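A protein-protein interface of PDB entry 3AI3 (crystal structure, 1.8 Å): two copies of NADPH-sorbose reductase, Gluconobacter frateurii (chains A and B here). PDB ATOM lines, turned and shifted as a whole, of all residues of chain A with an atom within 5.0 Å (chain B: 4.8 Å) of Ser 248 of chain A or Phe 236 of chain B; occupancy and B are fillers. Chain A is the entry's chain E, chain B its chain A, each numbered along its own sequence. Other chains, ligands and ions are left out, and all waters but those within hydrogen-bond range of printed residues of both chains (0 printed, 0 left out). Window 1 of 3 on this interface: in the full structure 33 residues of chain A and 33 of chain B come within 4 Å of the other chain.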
ATOM      1  N   ARG A 181       2.256   9.421 -21.740  1.00  0.00           N
ATOM      2  CA  ARG A 181       3.005   8.718 -20.688  1.00  0.00           C
ATOM      3  C   ARG A 181       2.892   7.231 -20.940  1.00  0.00           C
ATOM      4  O   ARG A 181       1.789   6.679 -20.956  1.00  0.00           O
ATOM      5  CB  ARG A 181       2.447   9.097 -19.321  1.00  0.00           C
ATOM      6  CG  ARG A 181       2.593  10.578 -19.035  1.00  0.00           C
ATOM      7  CD  ARG A 181       1.822  11.047 -17.791  1.00  0.00           C
ATOM      8  NE  ARG A 181       0.397  10.671 -17.795  1.00  0.00           N
ATOM      9  CZ  ARG A 181      -0.565  11.273 -18.507  1.00  0.00           C
ATOM     10  NH1 ARG A 181      -0.303  12.286 -19.344  1.00  0.00           N
ATOM     11  NH2 ARG A 181      -1.811  10.825 -18.422  1.00  0.00           N
ATOM     12  N   VAL A 182       4.030   6.590 -21.164  1.00  0.00           N
ATOM     13  CA  VAL A 182       4.052   5.173 -21.487  1.00  0.00           C
ATOM     14  C   VAL A 182       4.679   4.401 -20.346  1.00  0.00           C
ATOM     15  O   VAL A 182       5.747   4.770 -19.852  1.00  0.00           O
ATOM     16  CB  VAL A 182       4.879   4.920 -22.770  1.00  0.00           C
ATOM     17  CG1 VAL A 182       4.799   3.455 -23.223  1.00  0.00           C
ATOM     18  CG2 VAL A 182       4.434   5.830 -23.892  1.00  0.00           C
ATOM     19  N   ASN A 183       4.005   3.321 -19.929  1.00  0.00           N
ATOM     20  CA  ASN A 183       4.547   2.463 -18.874  1.00  0.00           C
ATOM     21  C   ASN A 183       4.198   1.013 -19.151  1.00  0.00           C
ATOM     22  O   ASN A 183       3.412   0.715 -20.028  1.00  0.00           O
ATOM     23  CB  ASN A 183       3.984   2.843 -17.492  1.00  0.00           C
ATOM     24  CG  ASN A 183       4.398   4.221 -17.062  1.00  0.00           C
ATOM     25  OD1 ASN A 183       5.524   4.424 -16.632  1.00  0.00           O
ATOM     26  ND2 ASN A 183       3.492   5.202 -17.231  1.00  0.00           N
ATOM     27  N   PHE A 236      -4.797  -1.422 -11.067  1.00  0.00           N
ATOM     28  CA  PHE A 236      -3.502  -0.811 -11.313  1.00  0.00           C
ATOM     29  C   PHE A 236      -3.426  -0.169 -12.692  1.00  0.00           C
ATOM     30  O   PHE A 236      -2.830   0.888 -12.845  1.00  0.00           O
ATOM     31  CB  PHE A 236      -2.394  -1.855 -11.151  1.00  0.00           C
ATOM     32  CG  PHE A 236      -1.133  -1.300 -10.556  1.00  0.00           C
ATOM     33  CD1 PHE A 236      -0.747  -1.674  -9.261  1.00  0.00           C
ATOM     34  CD2 PHE A 236      -0.332  -0.424 -11.280  1.00  0.00           C
ATOM     35  CE1 PHE A 236       0.429  -1.177  -8.706  1.00  0.00           C
ATOM     36  CE2 PHE A 236       0.841   0.085 -10.726  1.00  0.00           C
ATOM     37  CZ  PHE A 236       1.212  -0.303  -9.435  1.00  0.00           C
ATOM     38  N   PHE A 239      -5.476   3.112 -12.453  1.00  0.00           N
ATOM     39  CA  PHE A 239      -4.714   4.115 -11.750  1.00  0.00           C
ATOM     40  C   PHE A 239      -3.596   4.707 -12.617  1.00  0.00           C
ATOM     41  O   PHE A 239      -3.453   5.935 -12.700  1.00  0.00           O
ATOM     42  CB  PHE A 239      -4.168   3.548 -10.433  1.00  0.00           C
ATOM     43  CG  PHE A 239      -3.266   4.498  -9.726  1.00  0.00           C
ATOM     44  CD1 PHE A 239      -3.791   5.550  -9.010  1.00  0.00           C
ATOM     45  CD2 PHE A 239      -1.887   4.338  -9.790  1.00  0.00           C
ATOM     46  CE1 PHE A 239      -2.946   6.481  -8.364  1.00  0.00           C
ATOM     47  CE2 PHE A 239      -1.038   5.252  -9.180  1.00  0.00           C
ATOM     48  CZ  PHE A 239      -1.559   6.323  -8.464  1.00  0.00           C
ATOM     49  N   LEU A 240      -2.822   3.846 -13.277  1.00  0.00           N
ATOM     50  CA  LEU A 240      -1.674   4.334 -14.075  1.00  0.00           C
ATOM     51  C   LEU A 240      -2.135   5.197 -15.243  1.00  0.00           C
ATOM     52  O   LEU A 240      -1.404   6.088 -15.680  1.00  0.00           O
ATOM     53  CB  LEU A 240      -0.843   3.171 -14.637  1.00  0.00           C
ATOM     54  CG  LEU A 240       0.217   2.503 -13.780  1.00  0.00           C
ATOM     55  CD1 LEU A 240       1.118   1.779 -14.778  1.00  0.00           C
ATOM     56  CD2 LEU A 240       1.009   3.531 -12.978  1.00  0.00           C
ATOM     57  N   ALA A 245      -1.559   9.719 -11.863  1.00  0.00           N
ATOM     58  CA  ALA A 245      -0.253   9.064 -12.071  1.00  0.00           C
ATOM     59  C   ALA A 245       0.558   9.803 -13.128  1.00  0.00           C
ATOM     60  O   ALA A 245       1.161   9.197 -14.012  1.00  0.00           O
ATOM     61  CB  ALA A 245      -0.460   7.601 -12.466  1.00  0.00           C
ATOM     62  N   THR A 246       0.581  11.125 -13.020  1.00  0.00           N
ATOM     63  CA  THR A 246       1.119  11.964 -14.092  1.00  0.00           C
ATOM     64  C   THR A 246       2.658  12.054 -14.092  1.00  0.00           C
ATOM     65  O   THR A 246       3.234  12.714 -14.958  1.00  0.00           O
ATOM     66  CB  THR A 246       0.493  13.385 -14.075  1.00  0.00           C
ATOM     67  OG1 THR A 246       0.526  13.907 -12.737  1.00  0.00           O
ATOM     68  CG2 THR A 246      -0.978  13.335 -14.606  1.00  0.00           C
ATOM     69  N   TYR A 247       3.320  11.416 -13.131  1.00  0.00           N
ATOM     70  CA  TYR A 247       4.790  11.432 -13.128  1.00  0.00           C
ATOM     71  C   TYR A 247       5.378  10.074 -13.448  1.00  0.00           C
ATOM     72  O   TYR A 247       6.591   9.890 -13.407  1.00  0.00           O
ATOM     73  CB  TYR A 247       5.337  11.952 -11.793  1.00  0.00           C
ATOM     74  CG  TYR A 247       6.693  12.616 -11.923  1.00  0.00           C
ATOM     75  CD1 TYR A 247       6.829  13.824 -12.628  1.00  0.00           C
ATOM     76  CD2 TYR A 247       7.828  12.074 -11.317  1.00  0.00           C
ATOM     77  CE1 TYR A 247       8.038  14.457 -12.743  1.00  0.00           C
ATOM     78  CE2 TYR A 247       9.077  12.736 -11.418  1.00  0.00           C
ATOM     79  CZ  TYR A 247       9.168  13.902 -12.150  1.00  0.00           C
ATOM     80  OH  TYR A 247      10.371  14.555 -12.279  1.00  0.00           O
ATOM     81  N   SER A 248       4.513   9.123 -13.787  1.00  0.00           N
ATOM     82  CA  SER A 248       4.989   7.779 -14.163  1.00  0.00           C
ATOM     83  C   SER A 248       5.296   7.756 -15.650  1.00  0.00           C
ATOM     84  O   SER A 248       4.382   7.900 -16.459  1.00  0.00           O
ATOM     85  CB  SER A 248       3.933   6.735 -13.815  1.00  0.00           C
ATOM     86  OG  SER A 248       3.692   6.704 -12.409  1.00  0.00           O
ATOM     87  N   VAL A 249       6.575   7.618 -16.002  1.00  0.00           N
ATOM     88  CA  VAL A 249       7.058   7.654 -17.400  1.00  0.00           C
ATOM     89  C   VAL A 249       8.173   6.592 -17.536  1.00  0.00           C
ATOM     90  O   VAL A 249       9.158   6.615 -16.794  1.00  0.00           O
ATOM     91  CB  VAL A 249       7.671   9.058 -17.769  1.00  0.00           C
ATOM     92  CG1 VAL A 249       8.230   9.077 -19.205  1.00  0.00           C
ATOM     93  CG2 VAL A 249       6.637  10.174 -17.604  1.00  0.00           C
ATOM     94  N   GLY A 250       8.009   5.670 -18.476  1.00  0.00           N
ATOM     95  CA  GLY A 250       9.020   4.659 -18.766  1.00  0.00           C
ATOM     96  C   GLY A 250       9.329   3.710 -17.619  1.00  0.00           C
ATOM     97  O   GLY A 250      10.449   3.209 -17.501  1.00  0.00           O
ATOM     98  N   TYR A 253       6.031  -1.745 -13.686  1.00  0.00           N
ATOM     99  CA  TYR A 253       5.398  -1.949 -12.398  1.00  0.00           C
ATOM    100  C   TYR A 253       4.939  -3.380 -12.272  1.00  0.00           C
ATOM    101  O   TYR A 253       4.078  -3.825 -13.032  1.00  0.00           O
ATOM    102  CB  TYR A 253       4.190  -1.022 -12.272  1.00  0.00           C
ATOM    103  CG  TYR A 253       4.540   0.432 -12.257  1.00  0.00           C
ATOM    104  CD1 TYR A 253       5.340   0.952 -11.251  1.00  0.00           C
ATOM    105  CD2 TYR A 253       4.068   1.297 -13.229  1.00  0.00           C
ATOM    106  CE1 TYR A 253       5.675   2.316 -11.218  1.00  0.00           C
ATOM    107  CE2 TYR A 253       4.402   2.668 -13.206  1.00  0.00           C
ATOM    108  CZ  TYR A 253       5.175   3.163 -12.190  1.00  0.00           C
ATOM    109  OH  TYR A 253       5.519   4.497 -12.143  1.00  0.00           O
ATOM    110  N   ILE B 185       8.575   2.610  -2.675  1.00  0.00           N
ATOM    111  CA  ILE B 185       8.433   3.580  -3.765  1.00  0.00           C
ATOM    112  C   ILE B 185       9.758   4.329  -3.888  1.00  0.00           C
ATOM    113  O   ILE B 185      10.356   4.687  -2.886  1.00  0.00           O
ATOM    114  CB  ILE B 185       7.271   4.578  -3.527  1.00  0.00           C
ATOM    115  CG1 ILE B 185       5.929   3.878  -3.739  1.00  0.00           C
ATOM    116  CG2 ILE B 185       7.343   5.741  -4.491  1.00  0.00           C
ATOM    117  CD1 ILE B 185       4.716   4.750  -3.275  1.00  0.00           C
ATOM    118  N   GLU B 232       1.530  15.028  -6.499  1.00  0.00           N
ATOM    119  CA  GLU B 232       1.459  14.025  -7.546  1.00  0.00           C
ATOM    120  C   GLU B 232       2.126  12.723  -7.095  1.00  0.00           C
ATOM    121  O   GLU B 232       1.568  11.656  -7.304  1.00  0.00           O
ATOM    122  CB  GLU B 232       1.842  14.609  -8.924  1.00  0.00           C
ATOM    123  CG  GLU B 232       3.009  14.120  -9.682  1.00  0.00           C
ATOM    124  CD  GLU B 232       3.273  15.059 -10.873  1.00  0.00           C
ATOM    125  OE1 GLU B 232       2.847  14.779 -12.007  1.00  0.00           O
ATOM    126  OE2 GLU B 232       3.898  16.099 -10.672  1.00  0.00           O
ATOM    127  N   LEU B 233       3.243  12.813  -6.358  1.00  0.00           N
ATOM    128  CA  LEU B 233       3.848  11.604  -5.795  1.00  0.00           C
ATOM    129  C   LEU B 233       2.958  10.914  -4.761  1.00  0.00           C
ATOM    130  O   LEU B 233       2.829   9.670  -4.764  1.00  0.00           O
ATOM    131  CB  LEU B 233       5.197  11.926  -5.146  1.00  0.00           C
ATOM    132  CG  LEU B 233       5.901  10.747  -4.453  1.00  0.00           C
ATOM    133  CD1 LEU B 233       6.305   9.655  -5.482  1.00  0.00           C
ATOM    134  CD2 LEU B 233       7.125  11.287  -3.738  1.00  0.00           C
ATOM    135  N   ALA B 234       2.362  11.726  -3.880  1.00  0.00           N
ATOM    136  CA  ALA B 234       1.537  11.214  -2.788  1.00  0.00           C
ATOM    137  C   ALA B 234       0.421  10.312  -3.288  1.00  0.00           C
ATOM    138  O   ALA B 234       0.080   9.319  -2.616  1.00  0.00           O
ATOM    139  CB  ALA B 234       0.986  12.338  -1.967  1.00  0.00           C
ATOM    140  N   ASN B 235      -0.133  10.606  -4.467  1.00  0.00           N
ATOM    141  CA  ASN B 235      -1.183   9.728  -5.029  1.00  0.00           C
ATOM    142  C   ASN B 235      -0.757   8.272  -5.071  1.00  0.00           C
ATOM    143  O   ASN B 235      -1.557   7.386  -4.808  1.00  0.00           O
ATOM    144  CB  ASN B 235      -1.567  10.159  -6.442  1.00  0.00           C
ATOM    145  CG  ASN B 235      -2.184  11.539  -6.478  1.00  0.00           C
ATOM    146  OD1 ASN B 235      -2.895  11.924  -5.552  1.00  0.00           O
ATOM    147  ND2 ASN B 235      -1.925  12.290  -7.557  1.00  0.00           N
ATOM    148  N   PHE B 236       0.507   8.018  -5.408  1.00  0.00           N
ATOM    149  CA  PHE B 236       0.971   6.637  -5.552  1.00  0.00           C
ATOM    150  C   PHE B 236       1.042   5.929  -4.199  1.00  0.00           C
ATOM    151  O   PHE B 236       0.777   4.735  -4.106  1.00  0.00           O
ATOM    152  CB  PHE B 236       2.351   6.611  -6.226  1.00  0.00           C
ATOM    153  CG  PHE B 236       2.543   5.466  -7.197  1.00  0.00           C
ATOM    154  CD1 PHE B 236       2.542   5.696  -8.561  1.00  0.00           C
ATOM    155  CD2 PHE B 236       2.704   4.158  -6.735  1.00  0.00           C
ATOM    156  CE1 PHE B 236       2.716   4.652  -9.488  1.00  0.00           C
ATOM    157  CE2 PHE B 236       2.886   3.096  -7.633  1.00  0.00           C
ATOM    158  CZ  PHE B 236       2.903   3.341  -9.019  1.00  0.00           C
ATOM    159  N   PHE B 237       1.411   6.672  -3.151  1.00  0.00           N
ATOM    160  CA  PHE B 237       1.472   6.116  -1.801  1.00  0.00           C
ATOM    161  C   PHE B 237       0.070   5.721  -1.346  1.00  0.00           C
ATOM    162  O   PHE B 237      -0.133   4.659  -0.733  1.00  0.00           O
ATOM    163  CB  PHE B 237       2.072   7.140  -0.816  1.00  0.00           C
ATOM    164  CG  PHE B 237       3.580   7.238  -0.885  1.00  0.00           C
ATOM    165  CD1 PHE B 237       4.375   6.553   0.023  1.00  0.00           C
ATOM    166  CD2 PHE B 237       4.197   8.014  -1.875  1.00  0.00           C
ATOM    167  CE1 PHE B 237       5.776   6.633  -0.038  1.00  0.00           C
ATOM    168  CE2 PHE B 237       5.596   8.099  -1.964  1.00  0.00           C
ATOM    169  CZ  PHE B 237       6.395   7.402  -1.044  1.00  0.00           C
ATOM    170  N   VAL B 238      -0.886   6.597  -1.617  1.00  0.00           N
ATOM    171  CA  VAL B 238      -2.278   6.350  -1.204  1.00  0.00           C
ATOM    172  C   VAL B 238      -2.808   5.135  -1.940  1.00  0.00           C
ATOM    173  O   VAL B 238      -3.315   4.209  -1.301  1.00  0.00           O
ATOM    174  CB  VAL B 238      -3.175   7.572  -1.422  1.00  0.00           C
ATOM    175  CG1 VAL B 238      -4.589   7.274  -0.995  1.00  0.00           C
ATOM    176  CG2 VAL B 238      -2.655   8.781  -0.609  1.00  0.00           C
ATOM    177  N   PHE B 239      -2.627   5.097  -3.257  1.00  0.00           N
ATOM    178  CA  PHE B 239      -3.027   3.906  -4.024  1.00  0.00           C
ATOM    179  C   PHE B 239      -2.391   2.639  -3.472  1.00  0.00           C
ATOM    180  O   PHE B 239      -3.095   1.642  -3.224  1.00  0.00           O
ATOM    181  CB  PHE B 239      -2.727   4.073  -5.530  1.00  0.00           C
ATOM    182  CG  PHE B 239      -3.120   2.891  -6.337  1.00  0.00           C
ATOM    183  CD1 PHE B 239      -4.459   2.682  -6.665  1.00  0.00           C
ATOM    184  CD2 PHE B 239      -2.162   1.950  -6.714  1.00  0.00           C
ATOM    185  CE1 PHE B 239      -4.838   1.537  -7.402  1.00  0.00           C
ATOM    186  CE2 PHE B 239      -2.529   0.808  -7.442  1.00  0.00           C
ATOM    187  CZ  PHE B 239      -3.870   0.611  -7.785  1.00  0.00           C
ATOM    188  N   LEU B 240      -1.078   2.648  -3.252  1.00  0.00           N
ATOM    189  CA  LEU B 240      -0.419   1.412  -2.827  1.00  0.00           C
ATOM    190  C   LEU B 240      -0.862   0.914  -1.432  1.00  0.00           C
ATOM    191  O   LEU B 240      -0.849  -0.289  -1.163  1.00  0.00           O
ATOM    192  CB  LEU B 240       1.112   1.532  -2.951  1.00  0.00           C
ATOM    193  CG  LEU B 240       1.744   1.453  -4.351  1.00  0.00           C
ATOM    194  CD1 LEU B 240       3.259   1.480  -4.135  1.00  0.00           C
ATOM    195  CD2 LEU B 240       1.314   0.185  -5.210  1.00  0.00           C
ATOM    196  N   TYR B 253       8.338   0.420  -6.778  1.00  0.00           N
ATOM    197  CA  TYR B 253       7.669   1.203  -7.798  1.00  0.00           C
ATOM    198  C   TYR B 253       8.356   2.536  -7.964  1.00  0.00           C
ATOM    199  O   TYR B 253       8.356   3.368  -7.050  1.00  0.00           O
ATOM    200  CB  TYR B 253       6.215   1.449  -7.379  1.00  0.00           C
ATOM    201  CG  TYR B 253       5.419   0.161  -7.256  1.00  0.00           C
ATOM    202  CD1 TYR B 253       4.952  -0.492  -8.394  1.00  0.00           C
ATOM    203  CD2 TYR B 253       5.137  -0.397  -6.017  1.00  0.00           C
ATOM    204  CE1 TYR B 253       4.230  -1.676  -8.310  1.00  0.00           C
ATOM    205  CE2 TYR B 253       4.394  -1.586  -5.912  1.00  0.00           C
ATOM    206  CZ  TYR B 253       3.930  -2.206  -7.074  1.00  0.00           C
ATOM    207  OH  TYR B 253       3.216  -3.377  -7.032  1.00  0.00           O
ATOM    208  N   VAL B 255       8.721   6.312  -9.357  1.00  0.00           N
ATOM    209  CA  VAL B 255       7.832   7.366  -9.808  1.00  0.00           C
ATOM    210  C   VAL B 255       8.764   8.529 -10.129  1.00  0.00           C
ATOM    211  O   VAL B 255       9.078   9.315  -9.255  1.00  0.00           O
ATOM    212  CB  VAL B 255       6.839   7.770  -8.676  1.00  0.00           C
ATOM    213  CG1 VAL B 255       5.965   8.952  -9.129  1.00  0.00           C
ATOM    214  CG2 VAL B 255       5.985   6.536  -8.234  1.00  0.00           C
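Asn 183 of chain A touches none of the printed residues of chain B.
Of chain B, only Phe 236 comes within 4 Å of Ser 248 of chain A.
Printed residues of chain A within 4 Å of Asn 235 of chain B: Phe 239.
Phe 236 of chain B touches just these residues of chain A: Phe 239, Ser 248 and Tyr 253.
Of the printed residues of chain A, Leu 240 of chain B touches Phe 236.
Of the 13 printed residues of chain A, 6 touch a printed residue of chain B.
Hydrophobic or aromatic side chains of chain A that line the printed part of chain B: Phe 236, Phe 239, Tyr 247 and Tyr 253.
Along chain A the printed residues that touch a printed residue of chain B span positions 236 to 253.
Hydrophobic or aromatic side chains of chain B that line the printed part of chain A: Phe 236, Phe 239, Leu 240 and Tyr 253.
Among the printed residues, 12 pairs touch across the chains.
Among the printed residues, no Asp or Glu carboxylate lies within 4 Å of a Lys or Arg side-chain nitrogen of the other chain.
OE1 of Glu 232 of chain B is in hydrogen-bond range of OG1 of Thr 246 of chain A (2.6 Å).
Among the printed residues, pairs that only touch across the chains: Phe 236 of chain A with Phe 239 of chain B, Phe 236 of chain A with Leu 240 of chain B, Phe 236 of chain A with Tyr 253 of chain B, Phe 239 of chain A with Asn 235 of chain B, Phe 239 of chain A with Phe 236 of chain B, Phe 239 of chain A with Phe 239 of chain B, Tyr 247 of chain A with Glu 232 of chain B, Tyr 247 of chain A with Val 255 of chain B, Ser 248 of chain A with Phe 236 of chain B, Tyr 253 of chain A with Phe 236 of chain B and Tyr 253 of chain A with Tyr 253 of chain B.
Phe 236 of chain A touches Phe 239 of chain B, and with the chains exchanged Phe 239 of chain A touches Phe 236 of chain B.
Phe 236 of chain A touches Leu 240 of chain B, but with the chains exchanged Leu 240 of chain A does not touch Phe 236 of chain B (4.04 Å).
Phe 236 of chain A touches Tyr 253 of chain B, and with the chains exchanged Tyr 253 of chain A touches Phe 236 of chain B.
Phe 239 of chain B touches its own counterpart, Phe 239 of chain A.
Of the 12 pairs that touch across the chains among the printed residues, 6 have their exchanged pair printed and touching as well.
ND2 of Asn 183 of chain A lies within hydrogen-bond range of O of Ser 248 of chain A (2.9 Å).
OH of Tyr 253 of chain A is in hydrogen-bond range of OG of Ser 248 of chain A, 2.9 Å away.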
